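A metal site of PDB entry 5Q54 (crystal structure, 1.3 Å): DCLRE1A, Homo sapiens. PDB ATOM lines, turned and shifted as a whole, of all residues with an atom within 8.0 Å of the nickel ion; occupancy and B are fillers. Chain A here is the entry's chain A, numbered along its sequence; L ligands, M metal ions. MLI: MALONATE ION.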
ATOM      1  N   ASP A  18      16.292  11.679   6.463  1.00  0.00           N
ATOM      2  CA  ASP A  18      17.557  11.956   5.721  1.00  0.00           C
ATOM      3  C   ASP A  18      17.658  11.144   4.348  1.00  0.00           C
ATOM      4  O   ASP A  18      18.740  10.620   4.016  1.00  0.00           O
ATOM      5  CB  ASP A  18      18.764  11.851   6.611  1.00  0.00           C
ATOM      6  CG  ASP A  18      18.706  12.835   7.858  1.00  0.00           C
ATOM      7  OD1 ASP A  18      17.846  13.733   7.837  1.00  0.00           O
ATOM      8  OD2 ASP A  18      19.634  12.605   8.687  1.00  0.00           O
ATOM      9  N   THR A  34      17.172  15.769   9.683  1.00  0.00           N
ATOM     10  CA  THR A  34      17.729  15.966  11.032  1.00  0.00           C
ATOM     11  C   THR A  34      18.564  17.230  11.123  1.00  0.00           C
ATOM     12  O   THR A  34      18.601  17.902  12.182  1.00  0.00           O
ATOM     13  CB  THR A  34      18.512  14.765  11.520  1.00  0.00           C
ATOM     14  OG1 THR A  34      19.694  14.552  10.658  1.00  0.00           O
ATOM     15  CG2 THR A  34      17.691  13.510  11.626  1.00  0.00           C
ATOM     16  N   HIS A  35      19.322  17.586  10.080  1.00  0.00           N
ATOM     17  CA  HIS A  35      20.273  18.712  10.078  1.00  0.00           C
ATOM     18  C   HIS A  35      20.715  19.087   8.682  1.00  0.00           C
ATOM     19  O   HIS A  35      20.721  18.180   7.773  1.00  0.00           O
ATOM     20  CB  HIS A  35      21.418  18.457  11.101  1.00  0.00           C
ATOM     21  CG  HIS A  35      22.419  17.411  10.720  1.00  0.00           C
ATOM     22  ND1 HIS A  35      22.192  16.057  10.662  1.00  0.00           N
ATOM     23  CD2 HIS A  35      23.739  17.555  10.445  1.00  0.00           C
ATOM     24  CE1 HIS A  35      23.340  15.446  10.380  1.00  0.00           C
ATOM     25  NE2 HIS A  35      24.271  16.342  10.261  1.00  0.00           N
ATOM     26  N   PHE A  36      21.242  20.302   8.600  1.00  0.00           N
ATOM     27  CA  PHE A  36      21.763  20.817   7.277  1.00  0.00           C
ATOM     28  C   PHE A  36      23.230  20.487   7.016  1.00  0.00           C
ATOM     29  O   PHE A  36      24.083  21.467   6.982  1.00  0.00           O
ATOM     30  CB  PHE A  36      21.475  22.355   7.206  1.00  0.00           C
ATOM     31  CG  PHE A  36      21.588  22.940   5.805  1.00  0.00           C
ATOM     32  CD1 PHE A  36      20.517  22.750   4.930  1.00  0.00           C
ATOM     33  CD2 PHE A  36      22.647  23.763   5.421  1.00  0.00           C
ATOM     34  CE1 PHE A  36      20.548  23.320   3.621  1.00  0.00           C
ATOM     35  CE2 PHE A  36      22.722  24.267   4.099  1.00  0.00           C
ATOM     36  CZ  PHE A  36      21.684  24.128   3.248  1.00  0.00           C
ATOM     37  N   HIS A  37      23.562  19.205   6.857  1.00  0.00           N
ATOM     38  CA  HIS A  37      24.857  18.749   6.357  1.00  0.00           C
ATOM     39  C   HIS A  37      24.588  18.009   5.012  1.00  0.00           C
ATOM     40  O   HIS A  37      23.645  17.207   4.891  1.00  0.00           O
ATOM     41  CB  HIS A  37      25.619  17.859   7.348  1.00  0.00           C
ATOM     42  CG  HIS A  37      26.354  18.598   8.452  1.00  0.00           C
ATOM     43  ND1 HIS A  37      26.804  18.021   9.642  1.00  0.00           N
ATOM     44  CD2 HIS A  37      26.758  19.874   8.494  1.00  0.00           C
ATOM     45  CE1 HIS A  37      27.488  18.908  10.331  1.00  0.00           C
ATOM     46  NE2 HIS A  37      27.418  20.040   9.675  1.00  0.00           N
ATOM     47  N   SER A  38      25.512  18.200   4.055  1.00  0.00           N
ATOM     48  CA  SER A  38      25.267  17.793   2.647  1.00  0.00           C
ATOM     49  C   SER A  38      25.027  16.309   2.489  1.00  0.00           C
ATOM     50  O   SER A  38      24.151  15.985   1.685  1.00  0.00           O
ATOM     51  CB  SER A  38      26.316  18.399   1.686  1.00  0.00           C
ATOM     52  OG  SER A  38      27.605  17.926   1.982  1.00  0.00           O
ATOM     53  N   ASP A  39      25.701  15.430   3.214  1.00  0.00           N
ATOM     54  CA  ASP A  39      25.445  13.937   3.089  1.00  0.00           C
ATOM     55  C   ASP A  39      23.980  13.638   3.446  1.00  0.00           C
ATOM     56  O   ASP A  39      23.423  12.638   2.943  1.00  0.00           O
ATOM     57  CB  ASP A  39      26.386  13.072   3.883  1.00  0.00           C
ATOM     58  CG  ASP A  39      27.819  12.877   3.243  1.00  0.00           C
ATOM     59  OD1 ASP A  39      28.025  13.396   2.111  1.00  0.00           O
ATOM     60  OD2 ASP A  39      28.639  12.256   3.934  1.00  0.00           O
ATOM     61  N   HIS A  40      23.345  14.451   4.323  1.00  0.00           N
ATOM     62  CA  HIS A  40      21.993  14.204   4.814  1.00  0.00           C
ATOM     63  C   HIS A  40      20.959  14.888   4.006  1.00  0.00           C
ATOM     64  O   HIS A  40      19.862  14.269   3.762  1.00  0.00           O
ATOM     65  CB  HIS A  40      21.923  14.658   6.317  1.00  0.00           C
ATOM     66  CG  HIS A  40      22.822  13.878   7.185  1.00  0.00           C
ATOM     67  ND1 HIS A  40      22.396  12.846   7.995  1.00  0.00           N
ATOM     68  CD2 HIS A  40      24.173  13.923   7.341  1.00  0.00           C
ATOM     69  CE1 HIS A  40      23.425  12.282   8.589  1.00  0.00           C
ATOM     70  NE2 HIS A  40      24.527  12.922   8.207  1.00  0.00           N
ATOM     71  N   HIS A  96      24.887  18.744  18.047  1.00  0.00           N
ATOM     72  CA  HIS A  96      25.728  18.580  16.809  1.00  0.00           C
ATOM     73  C   HIS A  96      25.965  19.985  16.277  1.00  0.00           C
ATOM     74  O   HIS A  96      26.700  20.729  16.976  1.00  0.00           O
ATOM     75  CB  HIS A  96      25.035  17.602  15.869  1.00  0.00           C
ATOM     76  CG  HIS A  96      25.784  17.200  14.594  1.00  0.00           C
ATOM     77  ND1 HIS A  96      27.082  16.754  14.596  1.00  0.00           N
ATOM     78  CD2 HIS A  96      25.393  17.291  13.311  1.00  0.00           C
ATOM     79  CE1 HIS A  96      27.425  16.521  13.330  1.00  0.00           C
ATOM     80  NE2 HIS A  96      26.431  16.797  12.503  1.00  0.00           N
ATOM     81  N   CYS A  97      25.526  20.355  15.120  1.00  0.00           N
ATOM     82  CA  CYS A  97      25.631  21.730  14.552  1.00  0.00           C
ATOM     83  C   CYS A  97      24.346  22.511  14.837  1.00  0.00           C
ATOM     84  O   CYS A  97      23.332  21.939  15.258  1.00  0.00           O
ATOM     85  CB  CYS A  97      25.891  21.599  13.017  1.00  0.00           C
ATOM     86  SG  CYS A  97      24.565  20.825  12.055  1.00  0.00           S
ATOM     87  N   ALA A 100      20.456  21.060  14.504  1.00  0.00           N
ATOM     88  CA  ALA A 100      20.466  19.590  14.445  1.00  0.00           C
ATOM     89  C   ALA A 100      19.558  19.016  15.536  1.00  0.00           C
ATOM     90  O   ALA A 100      19.655  19.435  16.701  1.00  0.00           O
ATOM     91  CB  ALA A 100      21.866  19.043  14.550  1.00  0.00           C
ATOM     92  N   GLY A 117      19.858  11.135  14.556  1.00  0.00           N
ATOM     93  CA  GLY A 117      20.574  11.894  13.545  1.00  0.00           C
ATOM     94  C   GLY A 117      22.048  11.813  13.789  1.00  0.00           C
ATOM     95  O   GLY A 117      22.548  10.803  14.241  1.00  0.00           O
ATOM     96  N   ASP A 118      22.757  12.905  13.505  1.00  0.00           N
ATOM     97  CA  ASP A 118      24.158  13.095  14.032  1.00  0.00           C
ATOM     98  C   ASP A 118      24.120  13.749  15.426  1.00  0.00           C
ATOM     99  O   ASP A 118      23.327  14.703  15.589  1.00  0.00           O
ATOM    100  CB  ASP A 118      25.039  13.921  13.098  1.00  0.00           C
ATOM    101  CG  ASP A 118      25.506  13.207  11.864  1.00  0.00           C
ATOM    102  OD1 ASP A 118      25.418  11.973  11.748  1.00  0.00           O
ATOM    103  OD2 ASP A 118      26.127  13.910  11.048  1.00  0.00           O
ATOM    104  N   PHE A 119      24.855  13.224  16.390  1.00  0.00           N
ATOM    105  CA  PHE A 119      24.822  13.782  17.746  1.00  0.00           C
ATOM    106  C   PHE A 119      26.142  13.663  18.454  1.00  0.00           C
ATOM    107  O   PHE A 119      26.953  12.794  18.158  1.00  0.00           O
ATOM    108  CB  PHE A 119      23.624  13.216  18.613  1.00  0.00           C
ATOM    109  CG  PHE A 119      23.815  11.882  19.365  1.00  0.00           C
ATOM    110  CD1 PHE A 119      23.289  11.706  20.646  1.00  0.00           C
ATOM    111  CD2 PHE A 119      24.470  10.756  18.788  1.00  0.00           C
ATOM    112  CE1 PHE A 119      23.392  10.499  21.299  1.00  0.00           C
ATOM    113  CE2 PHE A 119      24.634   9.559  19.483  1.00  0.00           C
ATOM    114  CZ  PHE A 119      24.052   9.464  20.720  1.00  0.00           C
ATOM    115  N   ASP A 141      23.915   7.237  15.697  1.00  0.00           N
ATOM    116  CA  ASP A 141      25.137   7.814  15.029  1.00  0.00           C
ATOM    117  C   ASP A 141      26.320   7.143  15.693  1.00  0.00           C
ATOM    118  O   ASP A 141      26.779   7.445  16.788  1.00  0.00           O
ATOM    119  CB  ASP A 141      25.192   9.309  15.275  1.00  0.00           C
ATOM    120  CG  ASP A 141      26.528   9.948  14.898  1.00  0.00           C
ATOM    121  OD1 ASP A 141      27.353   9.260  14.232  1.00  0.00           O
ATOM    122  OD2 ASP A 141      26.743  11.126  15.314  1.00  0.00           O
ATOM    123  N   THR A 143      29.493   7.091  14.324  1.00  0.00           N
ATOM    124  CA  THR A 143      30.705   7.576  13.680  1.00  0.00           C
ATOM    125  C   THR A 143      31.948   7.160  14.360  1.00  0.00           C
ATOM    126  O   THR A 143      32.899   6.594  13.688  1.00  0.00           O
ATOM    127  CB  THR A 143      30.642   9.167  13.589  1.00  0.00           C
ATOM    128  OG1 THR A 143      29.562   9.585  12.761  1.00  0.00           O
ATOM    129  CG2 THR A 143      31.929   9.707  13.006  1.00  0.00           C
ATOM    130  N   SER A 183      31.191  23.769   6.118  1.00  0.00           N
ATOM    131  CA  SER A 183      29.833  23.371   6.464  1.00  0.00           C
ATOM    132  C   SER A 183      29.470  24.219   7.680  1.00  0.00           C
ATOM    133  O   SER A 183      30.358  24.844   8.291  1.00  0.00           O
ATOM    134  CB  SER A 183      29.703  21.868   6.849  1.00  0.00           C
ATOM    135  OG  SER A 183      30.519  21.586   7.980  1.00  0.00           O
ATOM    136  N   ILE A 184      28.227  24.232   8.066  1.00  0.00           N
ATOM    137  CA  ILE A 184      27.839  24.727   9.376  1.00  0.00           C
ATOM    138  C   ILE A 184      28.339  23.806  10.468  1.00  0.00           C
ATOM    139  O   ILE A 184      28.680  22.592  10.191  1.00  0.00           O
ATOM    140  CB  ILE A 184      26.321  24.958   9.568  1.00  0.00           C
ATOM    141  CG1 ILE A 184      25.486  23.694   9.477  1.00  0.00           C
ATOM    142  CG2 ILE A 184      25.841  25.979   8.534  1.00  0.00           C
ATOM    143  CD1 ILE A 184      24.065  23.870   9.958  1.00  0.00           C
ATOM    144  N   GLU A 296      31.981  17.419  16.895  1.00  0.00           N
ATOM    145  CA  GLU A 296      30.504  17.457  17.070  1.00  0.00           C
ATOM    146  C   GLU A 296      29.804  16.060  16.982  1.00  0.00           C
ATOM    147  O   GLU A 296      28.588  15.952  16.787  1.00  0.00           O
ATOM    148  CB  GLU A 296      29.849  18.495  16.205  1.00  0.00           C
ATOM    149  CG  GLU A 296      30.255  19.968  16.623  1.00  0.00           C
ATOM    150  CD  GLU A 296      29.560  21.101  15.851  1.00  0.00           C
ATOM    151  OE1 GLU A 296      29.070  20.906  14.710  1.00  0.00           O
ATOM    152  OE2 GLU A 296      29.608  22.267  16.440  1.00  0.00           O
ATOM    153  N   HIS A 297      30.635  15.028  17.152  1.00  0.00           N
ATOM    154  CA  HIS A 297      30.139  13.636  17.321  1.00  0.00           C
ATOM    155  C   HIS A 297      30.602  13.062  18.675  1.00  0.00           C
ATOM    156  O   HIS A 297      31.674  13.393  19.193  1.00  0.00           O
ATOM    157  CB  HIS A 297      30.613  12.691  16.164  1.00  0.00           C
ATOM    158  CG  HIS A 297      30.111  13.019  14.831  1.00  0.00           C
ATOM    159  ND1 HIS A 297      28.916  12.577  14.292  1.00  0.00           N
ATOM    160  CD2 HIS A 297      30.746  13.694  13.814  1.00  0.00           C
ATOM    161  CE1 HIS A 297      28.809  12.990  13.034  1.00  0.00           C
ATOM    162  NE2 HIS A 297      29.895  13.676  12.752  1.00  0.00           N
HETATM  163  C1  MLI L   1      29.072  15.499   8.439  1.00  0.00           C
HETATM  164  C2  MLI L   1      29.434  15.287   9.901  1.00  0.00           C
HETATM  165  C3  MLI L   1      27.756  14.839   8.006  1.00  0.00           C
HETATM  166  O6  MLI L   1      30.481  14.879  10.322  1.00  0.00           O
HETATM  167  O7  MLI L   1      28.557  15.605  10.706  1.00  0.00           O
HETATM  168  O8  MLI L   1      26.702  15.118   8.658  1.00  0.00           O
HETATM  169  O9  MLI L   1      27.708  14.285   6.847  1.00  0.00           O
HETATM  170 NI    NI M   1      26.431  16.016  10.449  1.00  0.00          NI
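OG1 of Thr 34 is in hydrogen-bond range of ND1 of His 35, at 2.9 Å. O of Ile 184 sits at hydrogen-bond distance from NE2 of His 37, 2.9 Å away. NE2 of His 37 is in hydrogen-bond range of SG of Cys 97. O of Glu 296 sits at hydrogen-bond distance from ND1 of His 96, at 2.8 Å. A ring nitrogen (NE2) of His 40 lies close to the side-chain carboxylate (OD2) of Asp 118.
The nickel ion is bound by an oxygen (O8) of the ligand (2.0 Å). O7 of the ligand binds the nickel ion, at 2.2 Å. The nickel ion is bound by NE2 of His 35, at 2.2 Å. The nickel ion is bound by ND1 of His 37. A ring nitrogen (NE2) of His 96 is bound to the nickel ion, 2.2 Å away. OD2 of Asp 118 is bound to the nickel ion (2.2 Å).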
